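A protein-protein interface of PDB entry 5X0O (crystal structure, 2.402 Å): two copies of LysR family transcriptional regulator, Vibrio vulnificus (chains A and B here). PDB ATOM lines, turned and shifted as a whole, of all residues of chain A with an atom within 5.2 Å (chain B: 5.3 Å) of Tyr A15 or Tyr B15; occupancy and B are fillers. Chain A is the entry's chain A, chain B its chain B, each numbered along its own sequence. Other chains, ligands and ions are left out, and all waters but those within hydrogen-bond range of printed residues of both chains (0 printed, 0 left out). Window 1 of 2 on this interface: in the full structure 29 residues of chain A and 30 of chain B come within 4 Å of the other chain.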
ATOM      1  N   THR A  13      28.555  -9.786 -26.558  1.00  0.00           N
ATOM      2  CA  THR A  13      27.839  -9.707 -27.821  1.00  0.00           C
ATOM      3  C   THR A  13      26.898  -8.515 -27.803  1.00  0.00           C
ATOM      4  O   THR A  13      26.491  -8.052 -26.731  1.00  0.00           O
ATOM      5  CB  THR A  13      27.040 -10.993 -28.090  1.00  0.00           C
ATOM      6  OG1 THR A  13      26.197 -11.280 -26.967  1.00  0.00           O
ATOM      7  CG2 THR A  13      27.976 -12.165 -28.333  1.00  0.00           C
ATOM      8  N   PRO A  14      26.540  -7.985 -28.978  1.00  0.00           N
ATOM      9  CA  PRO A  14      25.582  -6.874 -29.021  1.00  0.00           C
ATOM     10  C   PRO A  14      24.215  -7.299 -28.505  1.00  0.00           C
ATOM     11  O   PRO A  14      23.801  -8.451 -28.647  1.00  0.00           O
ATOM     12  CB  PRO A  14      25.531  -6.499 -30.507  1.00  0.00           C
ATOM     13  CG  PRO A  14      26.067  -7.689 -31.227  1.00  0.00           C
ATOM     14  CD  PRO A  14      27.075  -8.301 -30.312  1.00  0.00           C
ATOM     15  N   TYR A  15      23.511  -6.336 -27.913  1.00  0.00           N
ATOM     16  CA  TYR A  15      22.292  -6.593 -27.155  1.00  0.00           C
ATOM     17  C   TYR A  15      21.192  -7.238 -27.995  1.00  0.00           C
ATOM     18  O   TYR A  15      20.867  -8.415 -27.801  1.00  0.00           O
ATOM     19  CB  TYR A  15      21.791  -5.288 -26.535  1.00  0.00           C
ATOM     20  CG  TYR A  15      20.589  -5.446 -25.638  1.00  0.00           C
ATOM     21  CD1 TYR A  15      19.648  -4.430 -25.525  1.00  0.00           C
ATOM     22  CD2 TYR A  15      20.395  -6.607 -24.898  1.00  0.00           C
ATOM     23  CE1 TYR A  15      18.545  -4.567 -24.706  1.00  0.00           C
ATOM     24  CE2 TYR A  15      19.295  -6.754 -24.078  1.00  0.00           C
ATOM     25  CZ  TYR A  15      18.373  -5.730 -23.984  1.00  0.00           C
ATOM     26  OH  TYR A  15      17.275  -5.869 -23.167  1.00  0.00           O
ATOM     27  N   ASN A  16      20.607  -6.478 -28.924  1.00  0.00           N
ATOM     28  CA  ASN A  16      19.414  -6.960 -29.615  1.00  0.00           C
ATOM     29  C   ASN A  16      19.728  -8.087 -30.588  1.00  0.00           C
ATOM     30  O   ASN A  16      18.846  -8.898 -30.900  1.00  0.00           O
ATOM     31  CB  ASN A  16      18.731  -5.813 -30.357  1.00  0.00           C
ATOM     32  CG  ASN A  16      18.367  -4.661 -29.446  1.00  0.00           C
ATOM     33  OD1 ASN A  16      17.333  -4.684 -28.776  1.00  0.00           O
ATOM     34  ND2 ASN A  16      19.212  -3.637 -29.425  1.00  0.00           N
ATOM     35  N   LEU A  17      20.962  -8.163 -31.074  1.00  0.00           N
ATOM     36  CA  LEU A  17      21.302  -9.059 -32.170  1.00  0.00           C
ATOM     37  C   LEU A  17      21.827 -10.411 -31.706  1.00  0.00           C
ATOM     38  O   LEU A  17      22.069 -11.284 -32.548  1.00  0.00           O
ATOM     39  CB  LEU A  17      22.338  -8.391 -33.083  1.00  0.00           C
ATOM     40  CG  LEU A  17      22.062  -6.947 -33.511  1.00  0.00           C
ATOM     41  CD1 LEU A  17      23.256  -6.347 -34.244  1.00  0.00           C
ATOM     42  CD2 LEU A  17      20.820  -6.884 -34.378  1.00  0.00           C
ATOM     43  N   THR A  18      21.996 -10.612 -30.398  1.00  0.00           N
ATOM     44  CA  THR A  18      22.720 -11.785 -29.915  1.00  0.00           C
ATOM     45  C   THR A  18      22.014 -13.080 -30.300  1.00  0.00           C
ATOM     46  O   THR A  18      22.630 -13.991 -30.863  1.00  0.00           O
ATOM     47  CB  THR A  18      22.899 -11.704 -28.399  1.00  0.00           C
ATOM     48  OG1 THR A  18      23.826 -10.656 -28.086  1.00  0.00           O
ATOM     49  CG2 THR A  18      23.425 -13.030 -27.850  1.00  0.00           C
ATOM     50  N   THR A  42      25.382 -10.019 -22.857  1.00  0.00           N
ATOM     51  CA  THR A  42      24.819  -9.144 -23.879  1.00  0.00           C
ATOM     52  C   THR A  42      25.035  -7.689 -23.478  1.00  0.00           C
ATOM     53  O   THR A  42      24.635  -7.274 -22.384  1.00  0.00           O
ATOM     54  CB  THR A  42      23.333  -9.438 -24.077  1.00  0.00           C
ATOM     55  OG1 THR A  42      22.691  -9.572 -22.803  1.00  0.00           O
ATOM     56  CG2 THR A  42      23.150 -10.727 -24.857  1.00  0.00           C
ATOM     57  N   GLU A  43      25.666  -6.916 -24.358  1.00  0.00           N
ATOM     58  CA  GLU A  43      26.098  -5.557 -24.056  1.00  0.00           C
ATOM     59  C   GLU A  43      25.352  -4.555 -24.928  1.00  0.00           C
ATOM     60  O   GLU A  43      25.202  -4.760 -26.137  1.00  0.00           O
ATOM     61  CB  GLU A  43      27.611  -5.410 -24.262  1.00  0.00           C
ATOM     62  CG  GLU A  43      28.123  -3.982 -24.193  1.00  0.00           C
ATOM     63  CD  GLU A  43      27.761  -3.294 -22.892  1.00  0.00           C
ATOM     64  OE1 GLU A  43      27.938  -3.912 -21.821  1.00  0.00           O
ATOM     65  OE2 GLU A  43      27.297  -2.135 -22.939  1.00  0.00           O
ATOM     66  N   SER A  44      24.894  -3.463 -24.307  1.00  0.00           N
ATOM     67  CA  SER A  44      24.178  -2.426 -25.046  1.00  0.00           C
ATOM     68  C   SER A  44      25.122  -1.502 -25.809  1.00  0.00           C
ATOM     69  O   SER A  44      24.744  -0.974 -26.860  1.00  0.00           O
ATOM     70  CB  SER A  44      23.305  -1.604 -24.095  1.00  0.00           C
ATOM     71  OG  SER A  44      23.991  -0.447 -23.645  1.00  0.00           O
ATOM     72  N   ASN A 134      13.574   0.196 -24.357  1.00  0.00           N
ATOM     73  CA  ASN A 134      15.014  -0.001 -24.401  1.00  0.00           C
ATOM     74  C   ASN A 134      15.408  -1.359 -24.978  1.00  0.00           C
ATOM     75  O   ASN A 134      16.537  -1.809 -24.763  1.00  0.00           O
ATOM     76  CB  ASN A 134      15.612   0.179 -23.003  1.00  0.00           C
ATOM     77  CG  ASN A 134      15.018  -0.772 -21.983  1.00  0.00           C
ATOM     78  OD1 ASN A 134      13.930  -1.316 -22.179  1.00  0.00           O
ATOM     79  ND2 ASN A 134      15.731  -0.975 -20.879  1.00  0.00           N
ATOM     80  N   ALA A 135      14.504  -2.012 -25.705  1.00  0.00           N
ATOM     81  CA  ALA A 135      14.792  -3.287 -26.343  1.00  0.00           C
ATOM     82  C   ALA A 135      13.958  -3.389 -27.613  1.00  0.00           C
ATOM     83  O   ALA A 135      12.828  -2.898 -27.658  1.00  0.00           O
ATOM     84  CB  ALA A 135      14.500  -4.461 -25.401  1.00  0.00           C
ATOM     85  N   THR B  13       9.231  -2.858 -16.345  1.00  0.00           N
ATOM     86  CA  THR B  13       8.871  -4.267 -16.306  1.00  0.00           C
ATOM     87  C   THR B  13      10.111  -5.113 -16.059  1.00  0.00           C
ATOM     88  O   THR B  13      11.233  -4.677 -16.336  1.00  0.00           O
ATOM     89  CB  THR B  13       8.208  -4.715 -17.616  1.00  0.00           C
ATOM     90  OG1 THR B  13       9.003  -4.288 -18.728  1.00  0.00           O
ATOM     91  CG2 THR B  13       6.830  -4.103 -17.728  1.00  0.00           C
ATOM     92  N   PRO B  14       9.941  -6.330 -15.539  1.00  0.00           N
ATOM     93  CA  PRO B  14      11.098  -7.209 -15.335  1.00  0.00           C
ATOM     94  C   PRO B  14      11.754  -7.582 -16.656  1.00  0.00           C
ATOM     95  O   PRO B  14      11.101  -7.687 -17.696  1.00  0.00           O
ATOM     96  CB  PRO B  14      10.497  -8.437 -14.646  1.00  0.00           C
ATOM     97  CG  PRO B  14       9.218  -7.952 -14.055  1.00  0.00           C
ATOM     98  CD  PRO B  14       8.705  -6.919 -14.998  1.00  0.00           C
ATOM     99  N   TYR B  15      13.067  -7.806 -16.592  1.00  0.00           N
ATOM    100  CA  TYR B  15      13.864  -7.963 -17.806  1.00  0.00           C
ATOM    101  C   TYR B  15      13.428  -9.187 -18.608  1.00  0.00           C
ATOM    102  O   TYR B  15      13.059  -9.075 -19.782  1.00  0.00           O
ATOM    103  CB  TYR B  15      15.346  -8.043 -17.440  1.00  0.00           C
ATOM    104  CG  TYR B  15      16.257  -8.327 -18.610  1.00  0.00           C
ATOM    105  CD1 TYR B  15      16.072  -7.688 -19.831  1.00  0.00           C
ATOM    106  CD2 TYR B  15      17.307  -9.227 -18.494  1.00  0.00           C
ATOM    107  CE1 TYR B  15      16.903  -7.946 -20.905  1.00  0.00           C
ATOM    108  CE2 TYR B  15      18.147  -9.490 -19.563  1.00  0.00           C
ATOM    109  CZ  TYR B  15      17.940  -8.845 -20.766  1.00  0.00           C
ATOM    110  OH  TYR B  15      18.770  -9.099 -21.837  1.00  0.00           O
ATOM    111  N   ASN B  16      13.463 -10.367 -17.989  1.00  0.00           N
ATOM    112  CA  ASN B  16      13.222 -11.600 -18.729  1.00  0.00           C
ATOM    113  C   ASN B  16      11.750 -11.844 -19.039  1.00  0.00           C
ATOM    114  O   ASN B  16      11.446 -12.588 -19.976  1.00  0.00           O
ATOM    115  CB  ASN B  16      13.776 -12.799 -17.956  1.00  0.00           C
ATOM    116  CG  ASN B  16      15.282 -12.752 -17.806  1.00  0.00           C
ATOM    117  OD1 ASN B  16      16.018 -12.820 -18.792  1.00  0.00           O
ATOM    118  ND2 ASN B  16      15.752 -12.641 -16.567  1.00  0.00           N
ATOM    119  N   LEU B  17      10.834 -11.239 -18.288  1.00  0.00           N
ATOM    120  CA  LEU B  17       9.420 -11.577 -18.365  1.00  0.00           C
ATOM    121  C   LEU B  17       8.605 -10.595 -19.198  1.00  0.00           C
ATOM    122  O   LEU B  17       7.379 -10.718 -19.252  1.00  0.00           O
ATOM    123  CB  LEU B  17       8.825 -11.663 -16.958  1.00  0.00           C
ATOM    124  CG  LEU B  17       9.553 -12.539 -15.942  1.00  0.00           C
ATOM    125  CD1 LEU B  17       8.959 -12.355 -14.551  1.00  0.00           C
ATOM    126  CD2 LEU B  17       9.495 -13.995 -16.370  1.00  0.00           C
ATOM    127  N   THR B  18       9.249  -9.627 -19.851  1.00  0.00           N
ATOM    128  CA  THR B  18       8.487  -8.556 -20.487  1.00  0.00           C
ATOM    129  C   THR B  18       7.779  -9.035 -21.750  1.00  0.00           C
ATOM    130  O   THR B  18       6.602  -8.720 -21.962  1.00  0.00           O
ATOM    131  CB  THR B  18       9.400  -7.371 -20.801  1.00  0.00           C
ATOM    132  OG1 THR B  18       9.931  -6.840 -19.580  1.00  0.00           O
ATOM    133  CG2 THR B  18       8.623  -6.282 -21.517  1.00  0.00           C
ATOM    134  N   THR B  42      12.694  -2.156 -19.615  1.00  0.00           N
ATOM    135  CA  THR B  42      12.963  -3.458 -19.025  1.00  0.00           C
ATOM    136  C   THR B  42      14.141  -3.339 -18.069  1.00  0.00           C
ATOM    137  O   THR B  42      15.208  -2.845 -18.444  1.00  0.00           O
ATOM    138  CB  THR B  42      13.258  -4.490 -20.111  1.00  0.00           C
ATOM    139  OG1 THR B  42      14.329  -4.019 -20.939  1.00  0.00           O
ATOM    140  CG2 THR B  42      12.026  -4.725 -20.972  1.00  0.00           C
ATOM    141  N   GLU B  43      13.945  -3.777 -16.827  1.00  0.00           N
ATOM    142  CA  GLU B  43      14.939  -3.599 -15.778  1.00  0.00           C
ATOM    143  C   GLU B  43      15.191  -4.923 -15.077  1.00  0.00           C
ATOM    144  O   GLU B  43      14.245  -5.643 -14.737  1.00  0.00           O
ATOM    145  CB  GLU B  43      14.490  -2.535 -14.769  1.00  0.00           C
ATOM    146  CG  GLU B  43      15.444  -2.335 -13.598  1.00  0.00           C
ATOM    147  CD  GLU B  43      16.814  -1.816 -14.020  1.00  0.00           C
ATOM    148  OE1 GLU B  43      16.928  -1.219 -15.113  1.00  0.00           O
ATOM    149  OE2 GLU B  43      17.781  -2.008 -13.251  1.00  0.00           O
ATOM    150  N   SER B  44      16.469  -5.239 -14.859  1.00  0.00           N
ATOM    151  CA  SER B  44      16.860  -6.482 -14.210  1.00  0.00           C
ATOM    152  C   SER B  44      16.807  -6.408 -12.689  1.00  0.00           C
ATOM    153  O   SER B  44      16.972  -7.443 -12.033  1.00  0.00           O
ATOM    154  CB  SER B  44      18.271  -6.881 -14.651  1.00  0.00           C
ATOM    155  OG  SER B  44      18.808  -7.868 -13.788  1.00  0.00           O
ATOM    156  N   ASN B 134      23.696 -13.402 -18.989  1.00  0.00           N
ATOM    157  CA  ASN B 134      22.935 -12.418 -18.230  1.00  0.00           C
ATOM    158  C   ASN B 134      21.509 -12.263 -18.738  1.00  0.00           C
ATOM    159  O   ASN B 134      20.826 -11.311 -18.352  1.00  0.00           O
ATOM    160  CB  ASN B 134      23.644 -11.060 -18.251  1.00  0.00           C
ATOM    161  CG  ASN B 134      23.773 -10.490 -19.650  1.00  0.00           C
ATOM    162  OD1 ASN B 134      23.727 -11.222 -20.639  1.00  0.00           O
ATOM    163  ND2 ASN B 134      23.928  -9.171 -19.740  1.00  0.00           N
ATOM    164  N   ALA B 135      21.054 -13.173 -19.597  1.00  0.00           N
ATOM    165  CA  ALA B 135      19.706 -13.159 -20.144  1.00  0.00           C
ATOM    166  C   ALA B 135      19.217 -14.592 -20.278  1.00  0.00           C
ATOM    167  O   ALA B 135      19.967 -15.471 -20.709  1.00  0.00           O
ATOM    168  CB  ALA B 135      19.658 -12.465 -21.508  1.00  0.00           C
ATOM    169  N   ASN B 137      16.711 -15.683 -22.254  1.00  0.00           N
ATOM    170  CA  ASN B 137      16.257 -16.059 -23.590  1.00  0.00           C
ATOM    171  C   ASN B 137      17.346 -16.796 -24.360  1.00  0.00           C
ATOM    172  O   ASN B 137      17.057 -17.737 -25.110  1.00  0.00           O
ATOM    173  CB  ASN B 137      15.787 -14.820 -24.353  1.00  0.00           C
ATOM    174  CG  ASN B 137      16.924 -13.881 -24.708  1.00  0.00           C
ATOM    175  OD1 ASN B 137      17.923 -13.796 -23.994  1.00  0.00           O
ATOM    176  ND2 ASN B 137      16.768 -13.157 -25.810  1.00  0.00           N
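Tyr A15 touches its own counterpart, Tyr B15.
Thr A42 touches Asn B134, and with the chains exchanged Asn A134 touches Thr B42.
Of the 3 pairs that touch across the chains among the printed residues, 3 have their exchanged pair printed and touching as well.
The backbone NH (N) of Tyr A15 lies within hydrogen-bond range of the backbone carbonyl oxygen (O) of Glu A43 (2.9 Å).
The backbone carbonyl oxygen of Glu B43 sits at hydrogen-bond distance from the backbone NH of Tyr B15.
Tyr A15 touches just one residue of chain B: Tyr B15.
Leu A17 touches none of the printed residues of chain B.
Of the printed residues of chain B, Thr A42 touches Asn B134 (2.9 Å).
Of the printed residues of chain B, Asn A134 touches Thr B42.
Tyr B15 touches just one residue of chain A: Tyr A15.
Thr B18 touches none of the printed residues of chain A.
Printed residues of chain A within 4 Å of Thr B42: Asn A134.
Printed residues of chain A within 4 Å of Asn B134: Thr A42 (2.9 Å).
The nearest printed residue of chain A that does not touch Thr B42 is Tyr A15 (4.1 Å).
Of the 11 printed residues of chain A, 3 touch a printed residue of chain B.
Printed residues of chain A that touch a printed residue of chain B: Tyr A15, Thr A42 and Asn A134.
Printed residues of chain B that touch a printed residue of chain A: Tyr B15, Thr B42 and Asn B134.
Among the printed residues, 3 pairs touch across the chains.
Among the printed residues, no Asp or Glu carboxylate lies within 4 Å of a Lys or Arg side-chain nitrogen of the other chain.
Among the printed residues, pairs that only touch across the chains: Tyr A15 with Tyr B15.
The side-chain hydroxyl (OG1) of Thr A42 sits at hydrogen-bond distance from the side-chain amide oxygen (OD1) of Asn B134 (2.9 Å).
N of Thr B42 lies within hydrogen-bond range of OD1 of Asn A134, 3.0 Å away.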
